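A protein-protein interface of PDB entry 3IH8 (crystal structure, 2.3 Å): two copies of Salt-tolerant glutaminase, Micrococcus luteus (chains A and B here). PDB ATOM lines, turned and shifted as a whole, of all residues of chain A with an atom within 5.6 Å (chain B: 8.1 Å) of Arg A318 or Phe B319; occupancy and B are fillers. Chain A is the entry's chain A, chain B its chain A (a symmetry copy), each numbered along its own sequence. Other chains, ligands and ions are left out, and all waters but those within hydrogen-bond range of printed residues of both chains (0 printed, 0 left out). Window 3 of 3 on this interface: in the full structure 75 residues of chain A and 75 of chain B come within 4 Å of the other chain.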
ATOM      1  N   GLY A 314     -15.495 -12.445 -14.537  1.00  0.00           N
ATOM      2  CA  GLY A 314     -16.792 -11.917 -14.154  1.00  0.00           C
ATOM      3  C   GLY A 314     -17.264 -10.749 -14.993  1.00  0.00           C
ATOM      4  O   GLY A 314     -18.451 -10.413 -14.979  1.00  0.00           O
ATOM      5  N   THR A 315     -16.347 -10.128 -15.728  1.00  0.00           N
ATOM      6  CA  THR A 315     -16.714  -8.998 -16.567  1.00  0.00           C
ATOM      7  C   THR A 315     -17.641  -9.451 -17.697  1.00  0.00           C
ATOM      8  O   THR A 315     -18.161  -8.629 -18.458  1.00  0.00           O
ATOM      9  CB  THR A 315     -15.460  -8.312 -17.158  1.00  0.00           C
ATOM     10  OG1 THR A 315     -14.597  -7.911 -16.091  1.00  0.00           O
ATOM     11  CG2 THR A 315     -15.845  -7.074 -17.966  1.00  0.00           C
ATOM     12  N   ALA A 316     -17.857 -10.760 -17.794  1.00  0.00           N
ATOM     13  CA  ALA A 316     -18.741 -11.311 -18.820  1.00  0.00           C
ATOM     14  C   ALA A 316     -20.160 -10.815 -18.548  1.00  0.00           C
ATOM     15  O   ALA A 316     -20.980 -10.694 -19.457  1.00  0.00           O
ATOM     16  CB  ALA A 316     -18.707 -12.830 -18.784  1.00  0.00           C
ATOM     17  N   VAL A 317     -20.433 -10.532 -17.280  1.00  0.00           N
ATOM     18  CA  VAL A 317     -21.732 -10.037 -16.859  1.00  0.00           C
ATOM     19  C   VAL A 317     -21.657  -8.523 -16.804  1.00  0.00           C
ATOM     20  O   VAL A 317     -21.157  -7.960 -15.837  1.00  0.00           O
ATOM     21  CB  VAL A 317     -22.110 -10.598 -15.465  1.00  0.00           C
ATOM     22  CG1 VAL A 317     -23.404  -9.961 -14.964  1.00  0.00           C
ATOM     23  CG2 VAL A 317     -22.270 -12.116 -15.552  1.00  0.00           C
ATOM     24  N   ARG A 318     -22.139  -7.877 -17.863  1.00  0.00           N
ATOM     25  CA  ARG A 318     -22.136  -6.417 -17.977  1.00  0.00           C
ATOM     26  C   ARG A 318     -22.880  -5.757 -16.804  1.00  0.00           C
ATOM     27  O   ARG A 318     -22.412  -4.764 -16.241  1.00  0.00           O
ATOM     28  CB  ARG A 318     -22.766  -6.008 -19.319  1.00  0.00           C
ATOM     29  CG  ARG A 318     -22.500  -4.565 -19.733  1.00  0.00           C
ATOM     30  CD  ARG A 318     -23.151  -4.249 -21.071  1.00  0.00           C
ATOM     31  NE  ARG A 318     -23.019  -2.834 -21.421  1.00  0.00           N
ATOM     32  CZ  ARG A 318     -21.951  -2.286 -21.995  1.00  0.00           C
ATOM     33  NH1 ARG A 318     -20.896  -3.028 -22.306  1.00  0.00           N
ATOM     34  NH2 ARG A 318     -21.933  -0.984 -22.247  1.00  0.00           N
ATOM     35  N   PHE A 319     -24.036  -6.309 -16.440  1.00  0.00           N
ATOM     36  CA  PHE A 319     -24.822  -5.795 -15.318  1.00  0.00           C
ATOM     37  C   PHE A 319     -26.075  -6.623 -15.087  1.00  0.00           C
ATOM     38  O   PHE A 319     -26.497  -7.391 -15.955  1.00  0.00           O
ATOM     39  CB  PHE A 319     -25.232  -4.332 -15.536  1.00  0.00           C
ATOM     40  CG  PHE A 319     -26.164  -4.123 -16.697  1.00  0.00           C
ATOM     41  CD1 PHE A 319     -25.677  -4.083 -17.998  1.00  0.00           C
ATOM     42  CD2 PHE A 319     -27.531  -3.973 -16.487  1.00  0.00           C
ATOM     43  CE1 PHE A 319     -26.535  -3.896 -19.074  1.00  0.00           C
ATOM     44  CE2 PHE A 319     -28.400  -3.786 -17.556  1.00  0.00           C
ATOM     45  CZ  PHE A 319     -27.902  -3.746 -18.854  1.00  0.00           C
ATOM     46  N   VAL A 320     -26.664  -6.459 -13.906  1.00  0.00           N
ATOM     47  CA  VAL A 320     -27.880  -7.175 -13.541  1.00  0.00           C
ATOM     48  C   VAL A 320     -28.869  -6.199 -12.917  1.00  0.00           C
ATOM     49  O   VAL A 320     -28.545  -5.507 -11.950  1.00  0.00           O
ATOM     50  CB  VAL A 320     -27.590  -8.299 -12.530  1.00  0.00           C
ATOM     51  CG1 VAL A 320     -28.826  -9.158 -12.353  1.00  0.00           C
ATOM     52  CG2 VAL A 320     -26.427  -9.146 -13.008  1.00  0.00           C
ATOM     53  N   HIS A 330     -27.320  -8.868 -18.645  1.00  0.00           N
ATOM     54  CA  HIS A 330     -26.626  -8.619 -19.898  1.00  0.00           C
ATOM     55  C   HIS A 330     -25.202  -9.161 -19.873  1.00  0.00           C
ATOM     56  O   HIS A 330     -24.479  -9.012 -18.885  1.00  0.00           O
ATOM     57  CB  HIS A 330     -26.607  -7.120 -20.203  1.00  0.00           C
ATOM     58  CG  HIS A 330     -27.931  -6.578 -20.642  1.00  0.00           C
ATOM     59  ND1 HIS A 330     -29.050  -6.601 -19.839  1.00  0.00           N
ATOM     60  CD2 HIS A 330     -28.315  -6.003 -21.806  1.00  0.00           C
ATOM     61  CE1 HIS A 330     -30.067  -6.064 -20.488  1.00  0.00           C
ATOM     62  NE2 HIS A 330     -29.648  -5.694 -21.685  1.00  0.00           N
ATOM     63  N   LEU A 331     -24.810  -9.792 -20.976  1.00  0.00           N
ATOM     64  CA  LEU A 331     -23.480 -10.371 -21.107  1.00  0.00           C
ATOM     65  C   LEU A 331     -22.666  -9.584 -22.125  1.00  0.00           C
ATOM     66  O   LEU A 331     -23.216  -8.775 -22.874  1.00  0.00           O
ATOM     67  CB  LEU A 331     -23.585 -11.835 -21.547  1.00  0.00           C
ATOM     68  CG  LEU A 331     -24.562 -12.713 -20.764  1.00  0.00           C
ATOM     69  CD1 LEU A 331     -24.392 -14.156 -21.186  1.00  0.00           C
ATOM     70  CD2 LEU A 331     -24.314 -12.563 -19.275  1.00  0.00           C
ATOM     71  N   GLN A 332     -21.360  -9.828 -22.161  1.00  0.00           N
ATOM     72  CA  GLN A 332     -20.497  -9.118 -23.099  1.00  0.00           C
ATOM     73  C   GLN A 332     -19.128  -9.781 -23.222  1.00  0.00           C
ATOM     74  O   GLN A 332     -18.783 -10.660 -22.431  1.00  0.00           O
ATOM     75  CB  GLN A 332     -20.316  -7.676 -22.633  1.00  0.00           C
ATOM     76  CG  GLN A 332     -19.413  -7.545 -21.420  1.00  0.00           C
ATOM     77  CD  GLN A 332     -19.399  -6.149 -20.869  1.00  0.00           C
ATOM     78  OE1 GLN A 332     -19.719  -5.201 -21.574  1.00  0.00           O
ATOM     79  NE2 GLN A 332     -19.018  -6.007 -19.602  1.00  0.00           N
ATOM     80  N   ALA A 387     -19.774  -7.692 -12.706  1.00  0.00           N
ATOM     81  CA  ALA A 387     -21.115  -7.455 -12.178  1.00  0.00           C
ATOM     82  C   ALA A 387     -21.803  -8.736 -11.716  1.00  0.00           C
ATOM     83  O   ALA A 387     -23.034  -8.810 -11.687  1.00  0.00           O
ATOM     84  CB  ALA A 387     -21.974  -6.750 -13.230  1.00  0.00           C
ATOM     85  N   GLU A 390     -23.861  -8.354  -8.549  1.00  0.00           N
ATOM     86  CA  GLU A 390     -25.168  -7.722  -8.703  1.00  0.00           C
ATOM     87  C   GLU A 390     -26.270  -8.768  -8.773  1.00  0.00           C
ATOM     88  O   GLU A 390     -27.452  -8.433  -8.841  1.00  0.00           O
ATOM     89  CB  GLU A 390     -25.197  -6.866  -9.973  1.00  0.00           C
ATOM     90  CG  GLU A 390     -24.434  -5.556  -9.876  1.00  0.00           C
ATOM     91  CD  GLU A 390     -24.313  -4.853 -11.216  1.00  0.00           C
ATOM     92  OE1 GLU A 390     -25.338  -4.699 -11.917  1.00  0.00           O
ATOM     93  OE2 GLU A 390     -23.187  -4.448 -11.565  1.00  0.00           O
ATOM     94  N   ARG A 413     -24.295  -7.431 -26.577  1.00  0.00           N
ATOM     95  CA  ARG A 413     -22.936  -6.944 -26.350  1.00  0.00           C
ATOM     96  C   ARG A 413     -21.853  -8.022 -26.386  1.00  0.00           C
ATOM     97  O   ARG A 413     -20.664  -7.727 -26.290  1.00  0.00           O
ATOM     98  CB  ARG A 413     -22.882  -6.192 -25.017  1.00  0.00           C
ATOM     99  CG  ARG A 413     -23.594  -4.844 -25.040  1.00  0.00           C
ATOM    100  CD  ARG A 413     -22.737  -3.790 -25.718  1.00  0.00           C
ATOM    101  NE  ARG A 413     -23.451  -2.533 -25.925  1.00  0.00           N
ATOM    102  CZ  ARG A 413     -22.855  -1.381 -26.209  1.00  0.00           C
ATOM    103  NH1 ARG A 413     -21.534  -1.329 -26.313  1.00  0.00           N
ATOM    104  NH2 ARG A 413     -23.575  -0.284 -26.398  1.00  0.00           N
ATOM    105  N   GLY B 314     -10.649  -5.222 -26.112  1.00  0.00           N
ATOM    106  CA  GLY B 314     -11.500  -4.069 -26.344  1.00  0.00           C
ATOM    107  C   GLY B 314     -12.670  -3.952 -25.390  1.00  0.00           C
ATOM    108  O   GLY B 314     -13.276  -2.883 -25.279  1.00  0.00           O
ATOM    109  N   THR B 315     -12.991  -5.040 -24.697  1.00  0.00           N
ATOM    110  CA  THR B 315     -14.099  -5.015 -23.754  1.00  0.00           C
ATOM    111  C   THR B 315     -13.782  -4.084 -22.582  1.00  0.00           C
ATOM    112  O   THR B 315     -14.634  -3.831 -21.725  1.00  0.00           O
ATOM    113  CB  THR B 315     -14.415  -6.435 -23.229  1.00  0.00           C
ATOM    114  OG1 THR B 315     -14.692  -7.295 -24.337  1.00  0.00           O
ATOM    115  CG2 THR B 315     -15.634  -6.417 -22.309  1.00  0.00           C
ATOM    116  N   ALA B 316     -12.557  -3.565 -22.556  1.00  0.00           N
ATOM    117  CA  ALA B 316     -12.144  -2.645 -21.496  1.00  0.00           C
ATOM    118  C   ALA B 316     -12.983  -1.373 -21.611  1.00  0.00           C
ATOM    119  O   ALA B 316     -13.215  -0.671 -20.628  1.00  0.00           O
ATOM    120  CB  ALA B 316     -10.669  -2.308 -21.639  1.00  0.00           C
ATOM    121  N   VAL B 317     -13.430  -1.092 -22.828  1.00  0.00           N
ATOM    122  CA  VAL B 317     -14.253   0.074 -23.101  1.00  0.00           C
ATOM    123  C   VAL B 317     -15.705  -0.362 -23.060  1.00  0.00           C
ATOM    124  O   VAL B 317     -16.215  -0.917 -24.026  1.00  0.00           O
ATOM    125  CB  VAL B 317     -13.920   0.669 -24.492  1.00  0.00           C
ATOM    126  CG1 VAL B 317     -14.885   1.802 -24.835  1.00  0.00           C
ATOM    127  CG2 VAL B 317     -12.481   1.187 -24.494  1.00  0.00           C
ATOM    128  N   ARG B 318     -16.353  -0.124 -21.922  1.00  0.00           N
ATOM    129  CA  ARG B 318     -17.755  -0.488 -21.710  1.00  0.00           C
ATOM    130  C   ARG B 318     -18.672   0.152 -22.767  1.00  0.00           C
ATOM    131  O   ARG B 318     -19.571  -0.504 -23.299  1.00  0.00           O
ATOM    132  CB  ARG B 318     -18.184  -0.069 -20.294  1.00  0.00           C
ATOM    133  CG  ARG B 318     -19.482  -0.703 -19.808  1.00  0.00           C
ATOM    134  CD  ARG B 318     -19.826  -0.241 -18.400  1.00  0.00           C
ATOM    135  NE  ARG B 318     -21.134  -0.735 -17.968  1.00  0.00           N
ATOM    136  CZ  ARG B 318     -21.362  -1.940 -17.452  1.00  0.00           C
ATOM    137  NH1 ARG B 318     -20.368  -2.802 -17.285  1.00  0.00           N
ATOM    138  NH2 ARG B 318     -22.597  -2.290 -17.116  1.00  0.00           N
ATOM    139  N   PHE B 319     -18.442   1.429 -23.066  1.00  0.00           N
ATOM    140  CA  PHE B 319     -19.222   2.141 -24.078  1.00  0.00           C
ATOM    141  C   PHE B 319     -18.736   3.570 -24.256  1.00  0.00           C
ATOM    142  O   PHE B 319     -18.018   4.105 -23.408  1.00  0.00           O
ATOM    143  CB  PHE B 319     -20.715   2.168 -23.727  1.00  0.00           C
ATOM    144  CG  PHE B 319     -21.037   2.942 -22.479  1.00  0.00           C
ATOM    145  CD1 PHE B 319     -20.849   2.372 -21.225  1.00  0.00           C
ATOM    146  CD2 PHE B 319     -21.525   4.242 -22.559  1.00  0.00           C
ATOM    147  CE1 PHE B 319     -21.140   3.085 -20.068  1.00  0.00           C
ATOM    148  CE2 PHE B 319     -21.818   4.966 -21.408  1.00  0.00           C
ATOM    149  CZ  PHE B 319     -21.627   4.386 -20.159  1.00  0.00           C
ATOM    150  N   VAL B 320     -19.136   4.180 -25.367  1.00  0.00           N
ATOM    151  CA  VAL B 320     -18.762   5.555 -25.674  1.00  0.00           C
ATOM    152  C   VAL B 320     -19.995   6.318 -26.142  1.00  0.00           C
ATOM    153  O   VAL B 320     -20.671   5.902 -27.085  1.00  0.00           O
ATOM    154  CB  VAL B 320     -17.693   5.615 -26.780  1.00  0.00           C
ATOM    155  CG1 VAL B 320     -17.170   7.032 -26.907  1.00  0.00           C
ATOM    156  CG2 VAL B 320     -16.558   4.662 -26.463  1.00  0.00           C
ATOM    157  N   GLU B 321     -20.278   7.432 -25.471  1.00  0.00           N
ATOM    158  CA  GLU B 321     -21.433   8.265 -25.793  1.00  0.00           C
ATOM    159  C   GLU B 321     -21.064   9.709 -26.121  1.00  0.00           C
ATOM    160  O   GLU B 321     -20.211  10.312 -25.466  1.00  0.00           O
ATOM    161  CB  GLU B 321     -22.418   8.268 -24.623  1.00  0.00           C
ATOM    162  CG  GLU B 321     -23.085   6.935 -24.349  1.00  0.00           C
ATOM    163  CD  GLU B 321     -24.577   6.969 -24.627  1.00  0.00           C
ATOM    164  OE1 GLU B 321     -25.272   7.835 -24.049  1.00  0.00           O
ATOM    165  OE2 GLU B 321     -25.056   6.131 -25.419  1.00  0.00           O
ATOM    166  N   ARG B 322     -21.725  10.251 -27.138  1.00  0.00           N
ATOM    167  CA  ARG B 322     -21.515  11.629 -27.566  1.00  0.00           C
ATOM    168  C   ARG B 322     -22.851  12.348 -27.413  1.00  0.00           C
ATOM    169  O   ARG B 322     -23.662  12.366 -28.338  1.00  0.00           O
ATOM    170  CB  ARG B 322     -21.070  11.680 -29.030  1.00  0.00           C
ATOM    171  CG  ARG B 322     -20.803  13.088 -29.550  1.00  0.00           C
ATOM    172  CD  ARG B 322     -19.663  13.744 -28.786  1.00  0.00           C
ATOM    173  NE  ARG B 322     -19.364  15.088 -29.270  1.00  0.00           N
ATOM    174  CZ  ARG B 322     -19.012  15.373 -30.518  1.00  0.00           C
ATOM    175  NH1 ARG B 322     -18.756  16.625 -30.864  1.00  0.00           N
ATOM    176  NH2 ARG B 322     -18.918  14.409 -31.424  1.00  0.00           N
ATOM    177  N   VAL B 327     -17.804  13.890 -24.690  1.00  0.00           N
ATOM    178  CA  VAL B 327     -17.807  12.447 -24.910  1.00  0.00           C
ATOM    179  C   VAL B 327     -17.638  11.733 -23.576  1.00  0.00           C
ATOM    180  O   VAL B 327     -16.822  12.137 -22.742  1.00  0.00           O
ATOM    181  CB  VAL B 327     -16.648  12.011 -25.843  1.00  0.00           C
ATOM    182  CG1 VAL B 327     -16.603  10.492 -25.948  1.00  0.00           C
ATOM    183  CG2 VAL B 327     -16.828  12.620 -27.222  1.00  0.00           C
ATOM    184  N   PHE B 328     -18.415  10.674 -23.374  1.00  0.00           N
ATOM    185  CA  PHE B 328     -18.332   9.904 -22.141  1.00  0.00           C
ATOM    186  C   PHE B 328     -17.808   8.502 -22.424  1.00  0.00           C
ATOM    187  O   PHE B 328     -18.488   7.679 -23.041  1.00  0.00           O
ATOM    188  CB  PHE B 328     -19.701   9.832 -21.464  1.00  0.00           C
ATOM    189  CG  PHE B 328     -20.220  11.166 -21.013  1.00  0.00           C
ATOM    190  CD1 PHE B 328     -20.667  12.104 -21.937  1.00  0.00           C
ATOM    191  CD2 PHE B 328     -20.231  11.497 -19.663  1.00  0.00           C
ATOM    192  CE1 PHE B 328     -21.122  13.352 -21.524  1.00  0.00           C
ATOM    193  CE2 PHE B 328     -20.683  12.744 -19.238  1.00  0.00           C
ATOM    194  CZ  PHE B 328     -21.128  13.673 -20.171  1.00  0.00           C
ATOM    195  N   LEU B 329     -16.584   8.239 -21.975  1.00  0.00           N
ATOM    196  CA  LEU B 329     -15.967   6.942 -22.189  1.00  0.00           C
ATOM    197  C   LEU B 329     -15.832   6.191 -20.867  1.00  0.00           C
ATOM    198  O   LEU B 329     -15.110   6.615 -19.959  1.00  0.00           O
ATOM    199  CB  LEU B 329     -14.599   7.124 -22.856  1.00  0.00           C
ATOM    200  CG  LEU B 329     -14.078   5.968 -23.715  1.00  0.00           C
ATOM    201  CD1 LEU B 329     -12.928   6.442 -24.587  1.00  0.00           C
ATOM    202  CD2 LEU B 329     -13.646   4.823 -22.822  1.00  0.00           C
ATOM    203  N   HIS B 330     -16.550   5.078 -20.764  1.00  0.00           N
ATOM    204  CA  HIS B 330     -16.519   4.261 -19.561  1.00  0.00           C
ATOM    205  C   HIS B 330     -15.660   3.016 -19.746  1.00  0.00           C
ATOM    206  O   HIS B 330     -15.719   2.347 -20.780  1.00  0.00           O
ATOM    207  CB  HIS B 330     -17.939   3.859 -19.159  1.00  0.00           C
ATOM    208  CG  HIS B 330     -18.738   4.979 -18.571  1.00  0.00           C
ATOM    209  ND1 HIS B 330     -19.050   6.122 -19.274  1.00  0.00           N
ATOM    210  CD2 HIS B 330     -19.285   5.133 -17.341  1.00  0.00           C
ATOM    211  CE1 HIS B 330     -19.753   6.932 -18.505  1.00  0.00           C
ATOM    212  NE2 HIS B 330     -19.909   6.356 -17.326  1.00  0.00           N
ATOM    213  N   LEU B 331     -14.862   2.714 -18.726  1.00  0.00           N
ATOM    214  CA  LEU B 331     -13.976   1.559 -18.750  1.00  0.00           C
ATOM    215  C   LEU B 331     -14.456   0.512 -17.755  1.00  0.00           C
ATOM    216  O   LEU B 331     -15.305   0.797 -16.908  1.00  0.00           O
ATOM    217  CB  LEU B 331     -12.545   1.986 -18.402  1.00  0.00           C
ATOM    218  CG  LEU B 331     -11.994   3.197 -19.156  1.00  0.00           C
ATOM    219  CD1 LEU B 331     -10.520   3.353 -18.849  1.00  0.00           C
ATOM    220  CD2 LEU B 331     -12.210   3.021 -20.648  1.00  0.00           C
ATOM    221  N   GLN B 332     -13.909  -0.696 -17.849  1.00  0.00           N
ATOM    222  CA  GLN B 332     -14.311  -1.767 -16.943  1.00  0.00           C
ATOM    223  C   GLN B 332     -13.336  -2.940 -16.984  1.00  0.00           C
ATOM    224  O   GLN B 332     -12.472  -3.007 -17.860  1.00  0.00           O
ATOM    225  CB  GLN B 332     -15.704  -2.260 -17.325  1.00  0.00           C
ATOM    226  CG  GLN B 332     -15.722  -3.083 -18.599  1.00  0.00           C
ATOM    227  CD  GLN B 332     -17.118  -3.397 -19.054  1.00  0.00           C
ATOM    228  OE1 GLN B 332     -18.050  -3.366 -18.261  1.00  0.00           O
ATOM    229  NE2 GLN B 332     -17.275  -3.715 -20.337  1.00  0.00           N
ATOM    230  N   ALA B 346      -9.431   3.974 -28.414  1.00  0.00           N
ATOM    231  CA  ALA B 346     -10.668   4.734 -28.285  1.00  0.00           C
ATOM    232  C   ALA B 346     -10.374   6.229 -28.286  1.00  0.00           C
ATOM    233  O   ALA B 346     -10.982   6.995 -29.040  1.00  0.00           O
ATOM    234  CB  ALA B 346     -11.389   4.339 -27.005  1.00  0.00           C
ATOM    235  N   GLY B 386     -14.861  -5.043 -28.396  1.00  0.00           N
ATOM    236  CA  GLY B 386     -15.827  -4.442 -27.495  1.00  0.00           C
ATOM    237  C   GLY B 386     -16.469  -3.175 -28.033  1.00  0.00           C
ATOM    238  O   GLY B 386     -16.997  -3.159 -29.147  1.00  0.00           O
ATOM    239  N   ALA B 387     -16.419  -2.108 -27.240  1.00  0.00           N
ATOM    240  CA  ALA B 387     -17.011  -0.832 -27.632  1.00  0.00           C
ATOM    241  C   ALA B 387     -15.974   0.176 -28.119  1.00  0.00           C
ATOM    242  O   ALA B 387     -16.196   1.387 -28.046  1.00  0.00           O
ATOM    243  CB  ALA B 387     -17.805  -0.243 -26.465  1.00  0.00           C
ATOM    244  N   VAL B 388     -14.845  -0.325 -28.616  1.00  0.00           N
ATOM    245  CA  VAL B 388     -13.785   0.540 -29.125  1.00  0.00           C
ATOM    246  C   VAL B 388     -14.255   1.207 -30.417  1.00  0.00           C
ATOM    247  O   VAL B 388     -13.915   2.357 -30.700  1.00  0.00           O
ATOM    248  CB  VAL B 388     -12.484  -0.265 -29.394  1.00  0.00           C
ATOM    249  CG1 VAL B 388     -11.430   0.634 -30.032  1.00  0.00           C
ATOM    250  CG2 VAL B 388     -11.949  -0.841 -28.086  1.00  0.00           C
ATOM    251  N   HIS B 389     -15.055   0.474 -31.183  1.00  0.00           N
ATOM    252  CA  HIS B 389     -15.595   0.965 -32.444  1.00  0.00           C
ATOM    253  C   HIS B 389     -16.525   2.169 -32.255  1.00  0.00           C
ATOM    254  O   HIS B 389     -16.714   2.970 -33.173  1.00  0.00           O
ATOM    255  CB  HIS B 389     -16.345  -0.165 -33.164  1.00  0.00           C
ATOM    256  CG  HIS B 389     -17.461  -0.768 -32.363  1.00  0.00           C
ATOM    257  ND1 HIS B 389     -18.237  -1.805 -32.835  1.00  0.00           N
ATOM    258  CD2 HIS B 389     -17.936  -0.477 -31.128  1.00  0.00           C
ATOM    259  CE1 HIS B 389     -19.141  -2.124 -31.928  1.00  0.00           C
ATOM    260  NE2 HIS B 389     -18.980  -1.334 -30.882  1.00  0.00           N
ATOM    261  N   GLU B 390     -17.103   2.289 -31.063  1.00  0.00           N
ATOM    262  CA  GLU B 390     -18.010   3.390 -30.754  1.00  0.00           C
ATOM    263  C   GLU B 390     -17.252   4.706 -30.660  1.00  0.00           C
ATOM    264  O   GLU B 390     -17.850   5.764 -30.467  1.00  0.00           O
ATOM    265  CB  GLU B 390     -18.736   3.125 -29.432  1.00  0.00           C
ATOM    266  CG  GLU B 390     -19.832   2.076 -29.505  1.00  0.00           C
ATOM    267  CD  GLU B 390     -20.368   1.698 -28.136  1.00  0.00           C
ATOM    268  OE1 GLU B 390     -20.699   2.605 -27.340  1.00  0.00           O
ATOM    269  OE2 GLU B 390     -20.463   0.486 -27.859  1.00  0.00           O
ATOM    270  N   ALA B 391     -15.931   4.630 -30.788  1.00  0.00           N
ATOM    271  CA  ALA B 391     -15.081   5.810 -30.713  1.00  0.00           C
ATOM    272  C   ALA B 391     -15.110   6.569 -32.037  1.00  0.00           C
ATOM    273  O   ALA B 391     -15.243   7.792 -32.058  1.00  0.00           O
ATOM    274  CB  ALA B 391     -13.649   5.405 -30.363  1.00  0.00           C
ATOM    275  N   VAL B 408     -14.730  12.562 -20.660  1.00  0.00           N
ATOM    276  CA  VAL B 408     -14.885  12.082 -19.297  1.00  0.00           C
ATOM    277  C   VAL B 408     -14.560  10.599 -19.205  1.00  0.00           C
ATOM    278  O   VAL B 408     -15.236   9.771 -19.818  1.00  0.00           O
ATOM    279  CB  VAL B 408     -16.325  12.292 -18.794  1.00  0.00           C
ATOM    280  CG1 VAL B 408     -16.438  11.851 -17.343  1.00  0.00           C
ATOM    281  CG2 VAL B 408     -16.720  13.754 -18.939  1.00  0.00           C
ATOM    282  N   ASN B 410     -14.670   7.533 -16.989  1.00  0.00           N
ATOM    283  CA  ASN B 410     -15.282   6.984 -15.788  1.00  0.00           C
ATOM    284  C   ASN B 410     -14.665   5.618 -15.530  1.00  0.00           C
ATOM    285  O   ASN B 410     -14.692   4.742 -16.395  1.00  0.00           O
ATOM    286  CB  ASN B 410     -16.790   6.847 -15.969  1.00  0.00           C
ATOM    287  CG  ASN B 410     -17.476   6.317 -14.728  1.00  0.00           C
ATOM    288  OD1 ASN B 410     -17.212   5.199 -14.285  1.00  0.00           O
ATOM    289  ND2 ASN B 410     -18.363   7.122 -14.155  1.00  0.00           N
ATOM    290  N   ARG B 413     -16.540   1.265 -13.043  1.00  0.00           N
ATOM    291  CA  ARG B 413     -16.711  -0.153 -13.354  1.00  0.00           C
ATOM    292  C   ARG B 413     -15.408  -0.942 -13.485  1.00  0.00           C
ATOM    293  O   ARG B 413     -15.421  -2.158 -13.663  1.00  0.00           O
ATOM    294  CB  ARG B 413     -17.541  -0.297 -14.633  1.00  0.00           C
ATOM    295  CG  ARG B 413     -19.011   0.064 -14.457  1.00  0.00           C
ATOM    296  CD  ARG B 413     -19.771  -1.067 -13.786  1.00  0.00           C
ATOM    297  NE  ARG B 413     -21.138  -0.695 -13.434  1.00  0.00           N
ATOM    298  CZ  ARG B 413     -22.088  -1.570 -13.125  1.00  0.00           C
ATOM    299  NH1 ARG B 413     -21.817  -2.868 -13.132  1.00  0.00           N
ATOM    300  NH2 ARG B 413     -23.303  -1.152 -12.800  1.00  0.00           N
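Arg B318 touches its own counterpart, Arg A318.
Arg A318 touches Phe B319, and with the chains exchanged Phe A319 touches Arg B318.
Arg A318 touches Arg B413, and with the chains exchanged Arg A413 touches Arg B318.
Glu A390 touches Arg B413, and with the chains exchanged Arg A413 touches Glu B390.
Of the 13 printed residues of chain A, 6 touch a printed residue of chain B.
Hydrophobic or aromatic side chains of chain A that line the printed part of chain B: Phe A319 and Ala A387.
Of the 25 printed residues of chain B, 6 touch a printed residue of chain A.
Printed residues of chain B that touch a printed residue of chain A: Arg B318, Phe B319, Gln B332, Ala B387, Glu B390 and Arg B413.
Hydrophobic or aromatic side chains of chain B that line the printed part of chain A: Phe B319 and Ala B387.
Among the printed residues, Asp or Glu carboxylates within 4 Å of a Lys or Arg side-chain nitrogen of the other chain: Glu A390 with Arg B413 (2.6 Å) and Arg A413 with Glu B390 (2.6 Å).
Of chain B, only Arg B318 (2.6 Å), Phe B319 (3.7 Å) and Arg B413 (3.7 Å) come within 4 Å of Arg A318.
Of the printed residues of chain B, Ala A387 touches Arg B413.
Printed residues of chain B within 4 Å of Arg A413: Arg B318, Ala B387 and Glu B390.
Phe B319 touches just one residue of chain A: Arg A318.
Of the printed residues of chain A, Ala B387 touches Arg A413 (3.9 Å).
His B389 touches none of the printed residues of chain A.
Printed residues of chain A within 4 Å of Arg B413: Arg A318 (3.7 Å), Ala A387 (3.9 Å) and Glu A390 (2.6 Å).
The nearest residue of chain B that does not touch Arg A318 is Gln B332 (4.2 Å).
The nearest printed residue of chain B that does not touch Phe A319 is Arg B413 (4.4 Å).
The backbone carbonyl oxygen (O) of Ala A316 sits at hydrogen-bond distance from the backbone NH (N) of Gln A332.
The backbone carbonyl oxygen (O) of Val A317 sits close to the backbone NH (N) of Ala A387 (3.4 Å).
N of Arg A318 lies within hydrogen-bond range of O of His A330 (2.8 Å).
The backbone carbonyl oxygen (O) of Phe A319 sits at hydrogen-bond distance from the backbone NH (N) of His A330 (3.2 Å).
N of Val A320 is in hydrogen-bond range of OE1 of Glu A390 (3.0 Å).
The backbone NH (N) of Val B320 sits at hydrogen-bond distance from the side-chain carboxylate (OE1) of Glu B390, at 3.0 Å.
NH2 of Arg B318 sits at hydrogen-bond distance from O of Arg A318 (2.6 Å).
The side-chain amide nitrogen of Gln B332 lies close to the side-chain amide nitrogen of Gln A332 (3.0 Å).
OE2 of Glu A390 lies within salt-bridge range of NH1 of Arg B413.
The guanidinium group of Arg A413 is in salt-bridge range of the side-chain carboxylate of Glu B390, at 2.6 Å.
Among the printed residues, merely in contact across the chains: Arg A318 with Phe B319 (3.7 Å), Arg A318 with Arg B413 (3.7 Å), Phe A319 with Arg B318 (3.7 Å), Ala A387 with Arg B413 (3.9 Å), Arg A413 with Arg B318 (3.7 Å) and Arg A413 with Ala B387 (3.9 Å).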
